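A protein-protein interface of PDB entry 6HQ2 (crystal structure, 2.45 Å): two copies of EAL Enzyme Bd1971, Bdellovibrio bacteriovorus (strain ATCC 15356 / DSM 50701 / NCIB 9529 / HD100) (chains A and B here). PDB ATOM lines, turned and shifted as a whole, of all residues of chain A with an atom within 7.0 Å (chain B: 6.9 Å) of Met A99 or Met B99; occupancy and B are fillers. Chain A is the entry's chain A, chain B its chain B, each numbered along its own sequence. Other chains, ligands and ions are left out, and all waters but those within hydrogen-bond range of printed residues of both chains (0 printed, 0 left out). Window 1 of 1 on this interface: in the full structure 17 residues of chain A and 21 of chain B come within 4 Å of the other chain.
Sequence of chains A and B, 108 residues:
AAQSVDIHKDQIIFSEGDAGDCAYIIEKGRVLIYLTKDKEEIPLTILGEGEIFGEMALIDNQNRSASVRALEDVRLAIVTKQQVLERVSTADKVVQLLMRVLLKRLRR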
ATOM      1  N   VAL A  84     -27.372  20.608  13.860  1.00  0.00           N
ATOM      2  CA  VAL A  84     -26.843  19.479  13.154  1.00  0.00           C
ATOM      3  C   VAL A  84     -26.246  18.438  14.108  1.00  0.00           C
ATOM      4  O   VAL A  84     -26.615  17.265  14.049  1.00  0.00           O
ATOM      5  CB  VAL A  84     -25.802  19.932  12.138  1.00  0.00           C
ATOM      6  CG1 VAL A  84     -25.030  18.734  11.570  1.00  0.00           C
ATOM      7  CG2 VAL A  84     -26.532  20.698  11.052  1.00  0.00           C
ATOM      8  N   VAL A  88     -27.887  14.740  14.444  1.00  0.00           N
ATOM      9  CA  VAL A  88     -27.042  13.616  14.127  1.00  0.00           C
ATOM     10  C   VAL A  88     -26.915  12.685  15.342  1.00  0.00           C
ATOM     11  O   VAL A  88     -26.905  11.446  15.193  1.00  0.00           O
ATOM     12  CB  VAL A  88     -25.623  14.075  13.646  1.00  0.00           C
ATOM     13  CG1 VAL A  88     -24.656  12.896  13.559  1.00  0.00           C
ATOM     14  CG2 VAL A  88     -25.704  14.742  12.277  1.00  0.00           C
ATOM     15  N   ALA A  91     -29.986  10.485  15.721  1.00  0.00           N
ATOM     16  CA  ALA A  91     -30.277   9.686  14.551  1.00  0.00           C
ATOM     17  C   ALA A  91     -29.925   8.253  14.747  1.00  0.00           C
ATOM     18  O   ALA A  91     -29.270   7.861  15.734  1.00  0.00           O
ATOM     19  CB  ALA A  91     -29.525  10.229  13.344  1.00  0.00           C
ATOM     20  N   VAL A  94     -26.634   3.672  11.967  1.00  0.00           N
ATOM     21  CA  VAL A  94     -26.021   3.560  10.662  1.00  0.00           C
ATOM     22  C   VAL A  94     -25.968   4.904   9.979  1.00  0.00           C
ATOM     23  O   VAL A  94     -24.981   5.228   9.336  1.00  0.00           O
ATOM     24  CB  VAL A  94     -26.788   2.563   9.772  1.00  0.00           C
ATOM     25  CG1 VAL A  94     -26.355   2.655   8.298  1.00  0.00           C
ATOM     26  CG2 VAL A  94     -26.604   1.162  10.308  1.00  0.00           C
ATOM     27  N   VAL A  95     -27.031   5.686  10.105  1.00  0.00           N
ATOM     28  CA  VAL A  95     -27.066   7.026   9.535  1.00  0.00           C
ATOM     29  C   VAL A  95     -26.013   7.926  10.169  1.00  0.00           C
ATOM     30  O   VAL A  95     -25.354   8.662   9.474  1.00  0.00           O
ATOM     31  CB  VAL A  95     -28.458   7.639   9.659  1.00  0.00           C
ATOM     32  CG1 VAL A  95     -28.439   9.130   9.291  1.00  0.00           C
ATOM     33  CG2 VAL A  95     -29.433   6.884   8.740  1.00  0.00           C
ATOM     34  N   GLN A  96     -25.817   7.821  11.479  1.00  0.00           N
ATOM     35  CA  GLN A  96     -24.733   8.498  12.165  1.00  0.00           C
ATOM     36  C   GLN A  96     -23.393   8.224  11.562  1.00  0.00           C
ATOM     37  O   GLN A  96     -22.683   9.169  11.216  1.00  0.00           O
ATOM     38  CB  GLN A  96     -24.643   8.084  13.628  1.00  0.00           C
ATOM     39  CG  GLN A  96     -25.465   8.968  14.509  1.00  0.00           C
ATOM     40  CD  GLN A  96     -25.181   8.720  15.944  1.00  0.00           C
ATOM     41  OE1 GLN A  96     -24.204   8.118  16.253  1.00  0.00           O
ATOM     42  NE2 GLN A  96     -26.054   9.182  16.826  1.00  0.00           N
ATOM     43  N   LEU A  97     -23.028   6.946  11.480  1.00  0.00           N
ATOM     44  CA  LEU A  97     -21.702   6.546  10.973  1.00  0.00           C
ATOM     45  C   LEU A  97     -21.499   6.998   9.560  1.00  0.00           C
ATOM     46  O   LEU A  97     -20.400   7.354   9.175  1.00  0.00           O
ATOM     47  CB  LEU A  97     -21.525   5.027  10.963  1.00  0.00           C
ATOM     48  CG  LEU A  97     -21.427   4.304  12.283  1.00  0.00           C
ATOM     49  CD1 LEU A  97     -21.505   2.818  12.056  1.00  0.00           C
ATOM     50  CD2 LEU A  97     -20.117   4.677  12.963  1.00  0.00           C
ATOM     51  N   LEU A  98     -22.560   6.984   8.789  1.00  0.00           N
ATOM     52  CA  LEU A  98     -22.430   7.360   7.422  1.00  0.00           C
ATOM     53  C   LEU A  98     -22.209   8.880   7.299  1.00  0.00           C
ATOM     54  O   LEU A  98     -21.262   9.297   6.659  1.00  0.00           O
ATOM     55  CB  LEU A  98     -23.653   6.888   6.636  1.00  0.00           C
ATOM     56  CG  LEU A  98     -23.344   6.674   5.155  1.00  0.00           C
ATOM     57  CD1 LEU A  98     -22.037   5.927   4.969  1.00  0.00           C
ATOM     58  CD2 LEU A  98     -24.508   5.976   4.466  1.00  0.00           C
ATOM     59  N   MET A  99     -23.058   9.683   7.944  1.00  0.00           N
ATOM     60  CA  MET A  99     -22.920  11.143   8.015  1.00  0.00           C
ATOM     61  C   MET A  99     -21.527  11.528   8.482  1.00  0.00           C
ATOM     62  O   MET A  99     -20.851  12.348   7.876  1.00  0.00           O
ATOM     63  CB  MET A  99     -23.897  11.701   9.031  1.00  0.00           C
ATOM     64  CG  MET A  99     -25.357  11.756   8.618  1.00  0.00           C
ATOM     65  SD  MET A  99     -25.989  13.275   7.878  1.00  0.00           S
ATOM     66  CE  MET A  99     -25.056  14.530   8.717  1.00  0.00           C
ATOM     67  N   ARG A 100     -21.077  10.906   9.557  1.00  0.00           N
ATOM     68  CA  ARG A 100     -19.775  11.214  10.106  1.00  0.00           C
ATOM     69  C   ARG A 100     -18.625  10.961   9.158  1.00  0.00           C
ATOM     70  O   ARG A 100     -17.716  11.792   9.119  1.00  0.00           O
ATOM     71  CB  ARG A 100     -19.558  10.489  11.430  1.00  0.00           C
ATOM     72  CG  ARG A 100     -20.471  11.111  12.472  1.00  0.00           C
ATOM     73  CD  ARG A 100     -20.343  10.558  13.874  1.00  0.00           C
ATOM     74  NE  ARG A 100     -21.380  11.212  14.688  1.00  0.00           N
ATOM     75  CZ  ARG A 100     -21.794  10.759  15.866  1.00  0.00           C
ATOM     76  NH1 ARG A 100     -21.298   9.630  16.359  1.00  0.00           N
ATOM     77  NH2 ARG A 100     -22.734  11.419  16.524  1.00  0.00           N
ATOM     78  N   VAL A 101     -18.643   9.861   8.376  1.00  0.00           N
ATOM     79  CA  VAL A 101     -17.528   9.636   7.431  1.00  0.00           C
ATOM     80  C   VAL A 101     -17.695  10.465   6.159  1.00  0.00           C
ATOM     81  O   VAL A 101     -16.689  10.885   5.569  1.00  0.00           O
ATOM     82  CB  VAL A 101     -17.257   8.177   7.072  1.00  0.00           C
ATOM     83  CG1 VAL A 101     -16.945   7.398   8.314  1.00  0.00           C
ATOM     84  CG2 VAL A 101     -18.408   7.566   6.271  1.00  0.00           C
ATOM     85  N   LEU A 102     -18.934  10.779   5.789  1.00  0.00           N
ATOM     86  CA  LEU A 102     -19.168  11.600   4.618  1.00  0.00           C
ATOM     87  C   LEU A 102     -18.775  13.036   4.923  1.00  0.00           C
ATOM     88  O   LEU A 102     -18.104  13.661   4.116  1.00  0.00           O
ATOM     89  CB  LEU A 102     -20.595  11.447   4.090  1.00  0.00           C
ATOM     90  CG  LEU A 102     -20.976   9.990   3.728  1.00  0.00           C
ATOM     91  CD1 LEU A 102     -22.350   9.961   3.084  1.00  0.00           C
ATOM     92  CD2 LEU A 102     -19.991   9.273   2.821  1.00  0.00           C
ATOM     93  N   LEU A 103     -19.124  13.519   6.110  1.00  0.00           N
ATOM     94  CA  LEU A 103     -18.705  14.835   6.582  1.00  0.00           C
ATOM     95  C   LEU A 103     -17.196  14.936   6.613  1.00  0.00           C
ATOM     96  O   LEU A 103     -16.654  15.890   6.093  1.00  0.00           O
ATOM     97  CB  LEU A 103     -19.249  15.139   7.978  1.00  0.00           C
ATOM     98  CG  LEU A 103     -20.756  15.469   8.046  1.00  0.00           C
ATOM     99  CD1 LEU A 103     -21.265  15.568   9.483  1.00  0.00           C
ATOM    100  CD2 LEU A 103     -21.126  16.746   7.315  1.00  0.00           C
ATOM    101  N   LYS A 104     -16.497  13.970   7.194  1.00  0.00           N
ATOM    102  CA  LYS A 104     -15.052  14.016   7.140  1.00  0.00           C
ATOM    103  C   LYS A 104     -14.494  14.132   5.705  1.00  0.00           C
ATOM    104  O   LYS A 104     -13.535  14.881   5.467  1.00  0.00           O
ATOM    105  CB  LYS A 104     -14.443  12.779   7.745  1.00  0.00           C
ATOM    106  CG  LYS A 104     -14.465  12.645   9.248  1.00  0.00           C
ATOM    107  CD  LYS A 104     -13.578  11.422   9.596  1.00  0.00           C
ATOM    108  CE  LYS A 104     -13.443  11.052  11.078  1.00  0.00           C
ATOM    109  NZ  LYS A 104     -13.976  12.057  12.048  1.00  0.00           N
ATOM    110  N   ARG A 105     -15.055  13.366   4.761  1.00  0.00           N
ATOM    111  CA  ARG A 105     -14.523  13.326   3.378  1.00  0.00           C
ATOM    112  C   ARG A 105     -14.723  14.627   2.664  1.00  0.00           C
ATOM    113  O   ARG A 105     -13.882  15.078   1.888  1.00  0.00           O
ATOM    114  CB  ARG A 105     -15.223  12.266   2.543  1.00  0.00           C
ATOM    115  CG  ARG A 105     -14.786  10.863   2.841  1.00  0.00           C
ATOM    116  CD  ARG A 105     -15.387   9.924   1.816  1.00  0.00           C
ATOM    117  NE  ARG A 105     -14.306   9.517   0.947  1.00  0.00           N
ATOM    118  CZ  ARG A 105     -13.759   8.325   0.976  1.00  0.00           C
ATOM    119  NH1 ARG A 105     -14.238   7.383   1.778  1.00  0.00           N
ATOM    120  NH2 ARG A 105     -12.744   8.052   0.168  1.00  0.00           N
ATOM    121  N   ARG A 107     -15.031  17.663   4.188  1.00  0.00           N
ATOM    122  CA  ARG A 107     -14.198  18.688   4.784  1.00  0.00           C
ATOM    123  C   ARG A 107     -12.950  18.879   3.908  1.00  0.00           C
ATOM    124  O   ARG A 107     -12.545  20.027   3.648  1.00  0.00           O
ATOM    125  CB  ARG A 107     -13.813  18.352   6.245  1.00  0.00           C
ATOM    126  CG  ARG A 107     -14.679  19.016   7.327  1.00  0.00           C
ATOM    127  CD  ARG A 107     -16.127  18.562   7.223  1.00  0.00           C
ATOM    128  NE  ARG A 107     -17.085  19.068   8.226  1.00  0.00           N
ATOM    129  CZ  ARG A 107     -17.389  18.499   9.405  1.00  0.00           C
ATOM    130  NH1 ARG A 107     -16.795  17.387   9.833  1.00  0.00           N
ATOM    131  NH2 ARG A 107     -18.310  19.066  10.176  1.00  0.00           N
ATOM    132  N   ILE B  59     -22.246   5.732  -2.526  1.00  0.00           N
ATOM    133  CA  ILE B  59     -22.334   7.042  -3.159  1.00  0.00           C
ATOM    134  C   ILE B  59     -22.308   7.004  -4.697  1.00  0.00           C
ATOM    135  O   ILE B  59     -23.210   7.528  -5.337  1.00  0.00           O
ATOM    136  CB  ILE B  59     -21.261   8.033  -2.576  1.00  0.00           C
ATOM    137  CG1 ILE B  59     -21.854   8.831  -1.421  1.00  0.00           C
ATOM    138  CG2 ILE B  59     -20.747   9.051  -3.594  1.00  0.00           C
ATOM    139  CD1 ILE B  59     -21.852   8.119  -0.102  1.00  0.00           C
ATOM    140  N   VAL B  84     -29.789   2.070   3.390  1.00  0.00           N
ATOM    141  CA  VAL B  84     -29.530   3.474   3.584  1.00  0.00           C
ATOM    142  C   VAL B  84     -30.778   4.278   3.233  1.00  0.00           C
ATOM    143  O   VAL B  84     -31.220   5.103   4.014  1.00  0.00           O
ATOM    144  CB  VAL B  84     -28.322   3.913   2.742  1.00  0.00           C
ATOM    145  CG1 VAL B  84     -28.211   5.435   2.684  1.00  0.00           C
ATOM    146  CG2 VAL B  84     -27.056   3.293   3.317  1.00  0.00           C
ATOM    147  N   VAL B  88     -32.719   6.578   5.840  1.00  0.00           N
ATOM    148  CA  VAL B  88     -32.742   8.003   5.505  1.00  0.00           C
ATOM    149  C   VAL B  88     -34.191   8.504   5.383  1.00  0.00           C
ATOM    150  O   VAL B  88     -34.506   9.620   5.798  1.00  0.00           O
ATOM    151  CB  VAL B  88     -31.914   8.308   4.220  1.00  0.00           C
ATOM    152  CG1 VAL B  88     -32.201   9.692   3.672  1.00  0.00           C
ATOM    153  CG2 VAL B  88     -30.434   8.183   4.505  1.00  0.00           C
ATOM    154  N   ALA B  91     -35.732   9.157   8.797  1.00  0.00           N
ATOM    155  CA  ALA B  91     -34.924  10.049   9.598  1.00  0.00           C
ATOM    156  C   ALA B  91     -35.522  11.423   9.675  1.00  0.00           C
ATOM    157  O   ALA B  91     -36.473  11.764   8.964  1.00  0.00           O
ATOM    158  CB  ALA B  91     -33.515  10.151   9.022  1.00  0.00           C
ATOM    159  N   VAL B  94     -33.815  17.366   8.808  1.00  0.00           N
ATOM    160  CA  VAL B  94     -32.520  18.011   8.612  1.00  0.00           C
ATOM    161  C   VAL B  94     -31.446  16.982   8.270  1.00  0.00           C
ATOM    162  O   VAL B  94     -30.601  17.219   7.432  1.00  0.00           O
ATOM    163  CB  VAL B  94     -32.111  18.821   9.868  1.00  0.00           C
ATOM    164  CG1 VAL B  94     -30.642  19.232   9.818  1.00  0.00           C
ATOM    165  CG2 VAL B  94     -33.012  20.038  10.003  1.00  0.00           C
ATOM    166  N   VAL B  95     -31.480  15.851   8.945  1.00  0.00           N
ATOM    167  CA  VAL B  95     -30.571  14.766   8.631  1.00  0.00           C
ATOM    168  C   VAL B  95     -30.771  14.242   7.190  1.00  0.00           C
ATOM    169  O   VAL B  95     -29.796  13.981   6.490  1.00  0.00           O
ATOM    170  CB  VAL B  95     -30.698  13.636   9.662  1.00  0.00           C
ATOM    171  CG1 VAL B  95     -29.894  12.425   9.221  1.00  0.00           C
ATOM    172  CG2 VAL B  95     -30.201  14.137  11.027  1.00  0.00           C
ATOM    173  N   GLN B  96     -32.019  14.119   6.759  1.00  0.00           N
ATOM    174  CA  GLN B  96     -32.325  13.771   5.384  1.00  0.00           C
ATOM    175  C   GLN B  96     -31.683  14.695   4.381  1.00  0.00           C
ATOM    176  O   GLN B  96     -30.954  14.221   3.499  1.00  0.00           O
ATOM    177  CB  GLN B  96     -33.813  13.823   5.124  1.00  0.00           C
ATOM    178  CG  GLN B  96     -34.525  12.539   5.440  1.00  0.00           C
ATOM    179  CD  GLN B  96     -36.021  12.581   5.111  1.00  0.00           C
ATOM    180  OE1 GLN B  96     -36.532  13.564   4.586  1.00  0.00           O
ATOM    181  NE2 GLN B  96     -36.716  11.516   5.429  1.00  0.00           N
ATOM    182  N   LEU B  97     -31.961  15.996   4.506  1.00  0.00           N
ATOM    183  CA  LEU B  97     -31.411  16.974   3.582  1.00  0.00           C
ATOM    184  C   LEU B  97     -29.899  16.964   3.574  1.00  0.00           C
ATOM    185  O   LEU B  97     -29.262  17.240   2.564  1.00  0.00           O
ATOM    186  CB  LEU B  97     -31.851  18.380   3.935  1.00  0.00           C
ATOM    187  CG  LEU B  97     -33.314  18.689   3.739  1.00  0.00           C
ATOM    188  CD1 LEU B  97     -33.622  20.049   4.345  1.00  0.00           C
ATOM    189  CD2 LEU B  97     -33.667  18.679   2.270  1.00  0.00           C
ATOM    190  N   LEU B  98     -29.314  16.694   4.717  1.00  0.00           N
ATOM    191  CA  LEU B  98     -27.891  16.753   4.812  1.00  0.00           C
ATOM    192  C   LEU B  98     -27.255  15.568   4.124  1.00  0.00           C
ATOM    193  O   LEU B  98     -26.344  15.739   3.320  1.00  0.00           O
ATOM    194  CB  LEU B  98     -27.456  16.896   6.274  1.00  0.00           C
ATOM    195  CG  LEU B  98     -26.190  17.750   6.422  1.00  0.00           C
ATOM    196  CD1 LEU B  98     -26.328  19.117   5.728  1.00  0.00           C
ATOM    197  CD2 LEU B  98     -25.811  17.919   7.890  1.00  0.00           C
ATOM    198  N   MET B  99     -27.752  14.377   4.426  1.00  0.00           N
ATOM    199  CA  MET B  99     -27.356  13.157   3.698  1.00  0.00           C
ATOM    200  C   MET B  99     -27.439  13.366   2.193  1.00  0.00           C
ATOM    201  O   MET B  99     -26.516  13.069   1.444  1.00  0.00           O
ATOM    202  CB  MET B  99     -28.278  11.985   4.066  1.00  0.00           C
ATOM    203  CG  MET B  99     -27.889  11.290   5.365  1.00  0.00           C
ATOM    204  SD  MET B  99     -26.298  10.366   5.200  1.00  0.00           S
ATOM    205  CE  MET B  99     -26.595   9.508   3.644  1.00  0.00           C
ATOM    206  N   ARG B 100     -28.576  13.874   1.757  1.00  0.00           N
ATOM    207  CA  ARG B 100     -28.795  14.039   0.350  1.00  0.00           C
ATOM    208  C   ARG B 100     -27.803  14.976  -0.292  1.00  0.00           C
ATOM    209  O   ARG B 100     -27.417  14.731  -1.408  1.00  0.00           O
ATOM    210  CB  ARG B 100     -30.235  14.440   0.095  1.00  0.00           C
ATOM    211  CG  ARG B 100     -31.197  13.298   0.423  1.00  0.00           C
ATOM    212  CD  ARG B 100     -32.627  13.688   0.034  1.00  0.00           C
ATOM    213  NE  ARG B 100     -33.700  13.134   0.883  1.00  0.00           N
ATOM    214  CZ  ARG B 100     -34.014  11.842   1.070  1.00  0.00           C
ATOM    215  NH1 ARG B 100     -33.320  10.860   0.500  1.00  0.00           N
ATOM    216  NH2 ARG B 100     -35.029  11.524   1.880  1.00  0.00           N
ATOM    217  N   VAL B 101     -27.363  16.036   0.379  1.00  0.00           N
ATOM    218  CA  VAL B 101     -26.366  16.889  -0.267  1.00  0.00           C
ATOM    219  C   VAL B 101     -24.959  16.322  -0.150  1.00  0.00           C
ATOM    220  O   VAL B 101     -24.120  16.588  -0.985  1.00  0.00           O
ATOM    221  CB  VAL B 101     -26.408  18.379   0.153  1.00  0.00           C
ATOM    222  CG1 VAL B 101     -27.786  18.957  -0.149  1.00  0.00           C
ATOM    223  CG2 VAL B 101     -26.002  18.573   1.595  1.00  0.00           C
ATOM    224  N   LEU B 102     -24.679  15.544   0.875  1.00  0.00           N
ATOM    225  CA  LEU B 102     -23.393  14.834   0.911  1.00  0.00           C
ATOM    226  C   LEU B 102     -23.231  13.866  -0.267  1.00  0.00           C
ATOM    227  O   LEU B 102     -22.204  13.858  -0.947  1.00  0.00           O
ATOM    228  CB  LEU B 102     -23.255  14.059   2.226  1.00  0.00           C
ATOM    229  CG  LEU B 102     -23.020  14.928   3.466  1.00  0.00           C
ATOM    230  CD1 LEU B 102     -22.996  14.084   4.706  1.00  0.00           C
ATOM    231  CD2 LEU B 102     -21.742  15.747   3.408  1.00  0.00           C
ATOM    232  N   LEU B 103     -24.251  13.044  -0.496  1.00  0.00           N
ATOM    233  CA  LEU B 103     -24.318  12.189  -1.682  1.00  0.00           C
ATOM    234  C   LEU B 103     -24.152  12.982  -2.974  1.00  0.00           C
ATOM    235  O   LEU B 103     -23.351  12.607  -3.804  1.00  0.00           O
ATOM    236  CB  LEU B 103     -25.632  11.380  -1.698  1.00  0.00           C
ATOM    237  CG  LEU B 103     -25.768  10.139  -0.736  1.00  0.00           C
ATOM    238  CD1 LEU B 103     -24.948  10.228   0.553  1.00  0.00           C
ATOM    239  CD2 LEU B 103     -27.200   9.800  -0.339  1.00  0.00           C
ATOM    240  N   LYS B 104     -24.866  14.087  -3.133  1.00  0.00           N
ATOM    241  CA  LYS B 104     -24.668  14.958  -4.310  1.00  0.00           C
ATOM    242  C   LYS B 104     -23.205  15.404  -4.501  1.00  0.00           C
ATOM    243  O   LYS B 104     -22.661  15.348  -5.621  1.00  0.00           O
ATOM    244  CB  LYS B 104     -25.605  16.187  -4.278  1.00  0.00           C
ATOM    245  CG  LYS B 104     -25.375  17.198  -5.411  1.00  0.00           C
ATOM    246  CD  LYS B 104     -26.520  18.212  -5.676  1.00  0.00           C
ATOM    247  CE  LYS B 104     -26.844  19.187  -4.543  1.00  0.00           C
ATOM    248  NZ  LYS B 104     -25.720  19.756  -3.733  1.00  0.00           N
ATOM    249  N   ARG B 105     -22.563  15.838  -3.421  1.00  0.00           N
ATOM    250  CA  ARG B 105     -21.269  16.481  -3.573  1.00  0.00           C
ATOM    251  C   ARG B 105     -20.147  15.490  -3.728  1.00  0.00           C
ATOM    252  O   ARG B 105     -19.211  15.759  -4.469  1.00  0.00           O
ATOM    253  CB  ARG B 105     -20.961  17.423  -2.426  1.00  0.00           C
ATOM    254  CG  ARG B 105     -21.649  18.738  -2.639  1.00  0.00           C
ATOM    255  CD  ARG B 105     -21.518  19.632  -1.456  1.00  0.00           C
ATOM    256  NE  ARG B 105     -22.579  20.594  -1.567  1.00  0.00           N
ATOM    257  CZ  ARG B 105     -22.447  21.833  -1.997  1.00  0.00           C
ATOM    258  NH1 ARG B 105     -21.264  22.332  -2.301  1.00  0.00           N
ATOM    259  NH2 ARG B 105     -23.521  22.591  -2.100  1.00  0.00           N
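Printed residues of chain A that touch a printed residue of chain B: Val A84, Val A95, Leu A98, Met A99 and Leu A102. Hydrophobic or aromatic side chains of chain A within 4 Å of the printed part of chain B: Val A84, Val A95, Leu A98, Met A99 and Leu A102. Hydrophobic or aromatic side chains of chain B within 4 Å of the printed part of chain A: Ile B59, Val B84, Val B95, Leu B98, Met B99, Leu B102 and Leu B103. Among the printed residues, no Asp or Glu carboxylate lies within 4 Å of a Lys or Arg side-chain nitrogen of the other chain.
Met A99 touches Leu B98, but with the chains exchanged Leu A98 does not touch Met B99 (4.2 Å). Met B99 touches its own counterpart, Met A99. Leu B102 touches its own counterpart, Leu A102. Leu A102 touches Leu B103, but with the chains exchanged Leu A103 does not touch Leu B102 (4.1 Å). Positions printed for both chains: 84, 88, 91, 94, 95, 96, 97, 98, 99, 100, 101, 102, 103, 104 and 105. Of the 8 pairs that touch across the chains among the printed residues, 5 have their exchanged pair printed and touching as well.
Met A99 touches just these residues of chain B: Leu B98 (3.6 Å) and Met B99 (3.7 Å). Of chain A, only Met A99 (3.7 Å) comes within 4 Å of Met B99. Of the printed residues of chain A, Leu B102 touches Leu A102. Of the printed residues of chain A, Ile B59 touches Leu A102 (3.7 Å). Printed residues of chain A within 4 Å of Val B95: Val A95. Printed residues of chain A within 4 Å of Leu B98: Val A84 (3.8 Å) and Met A99 (3.6 Å). Of the printed residues of chain A, Leu B103 touches Leu A102 (3.6 Å). The nearest residue of chain B that does not touch Met A99 is Val B95 (4.1 Å). The nearest residue of chain A that does not touch Met B99 is Leu A98 (4.2 Å). The nearest printed residue of chain A that does not touch Leu B102 is Leu A103 (4.1 Å).
Among the printed residues, pairs that only touch across the chains: Val A84 with Leu B98, Val A95 with Val B95, Leu A98 with Val B84, Met A99 with Leu B98, Met A99 with Met B99, Leu A102 with Ile B59, Leu A102 with Leu B102 and Leu A102 with Leu B103.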
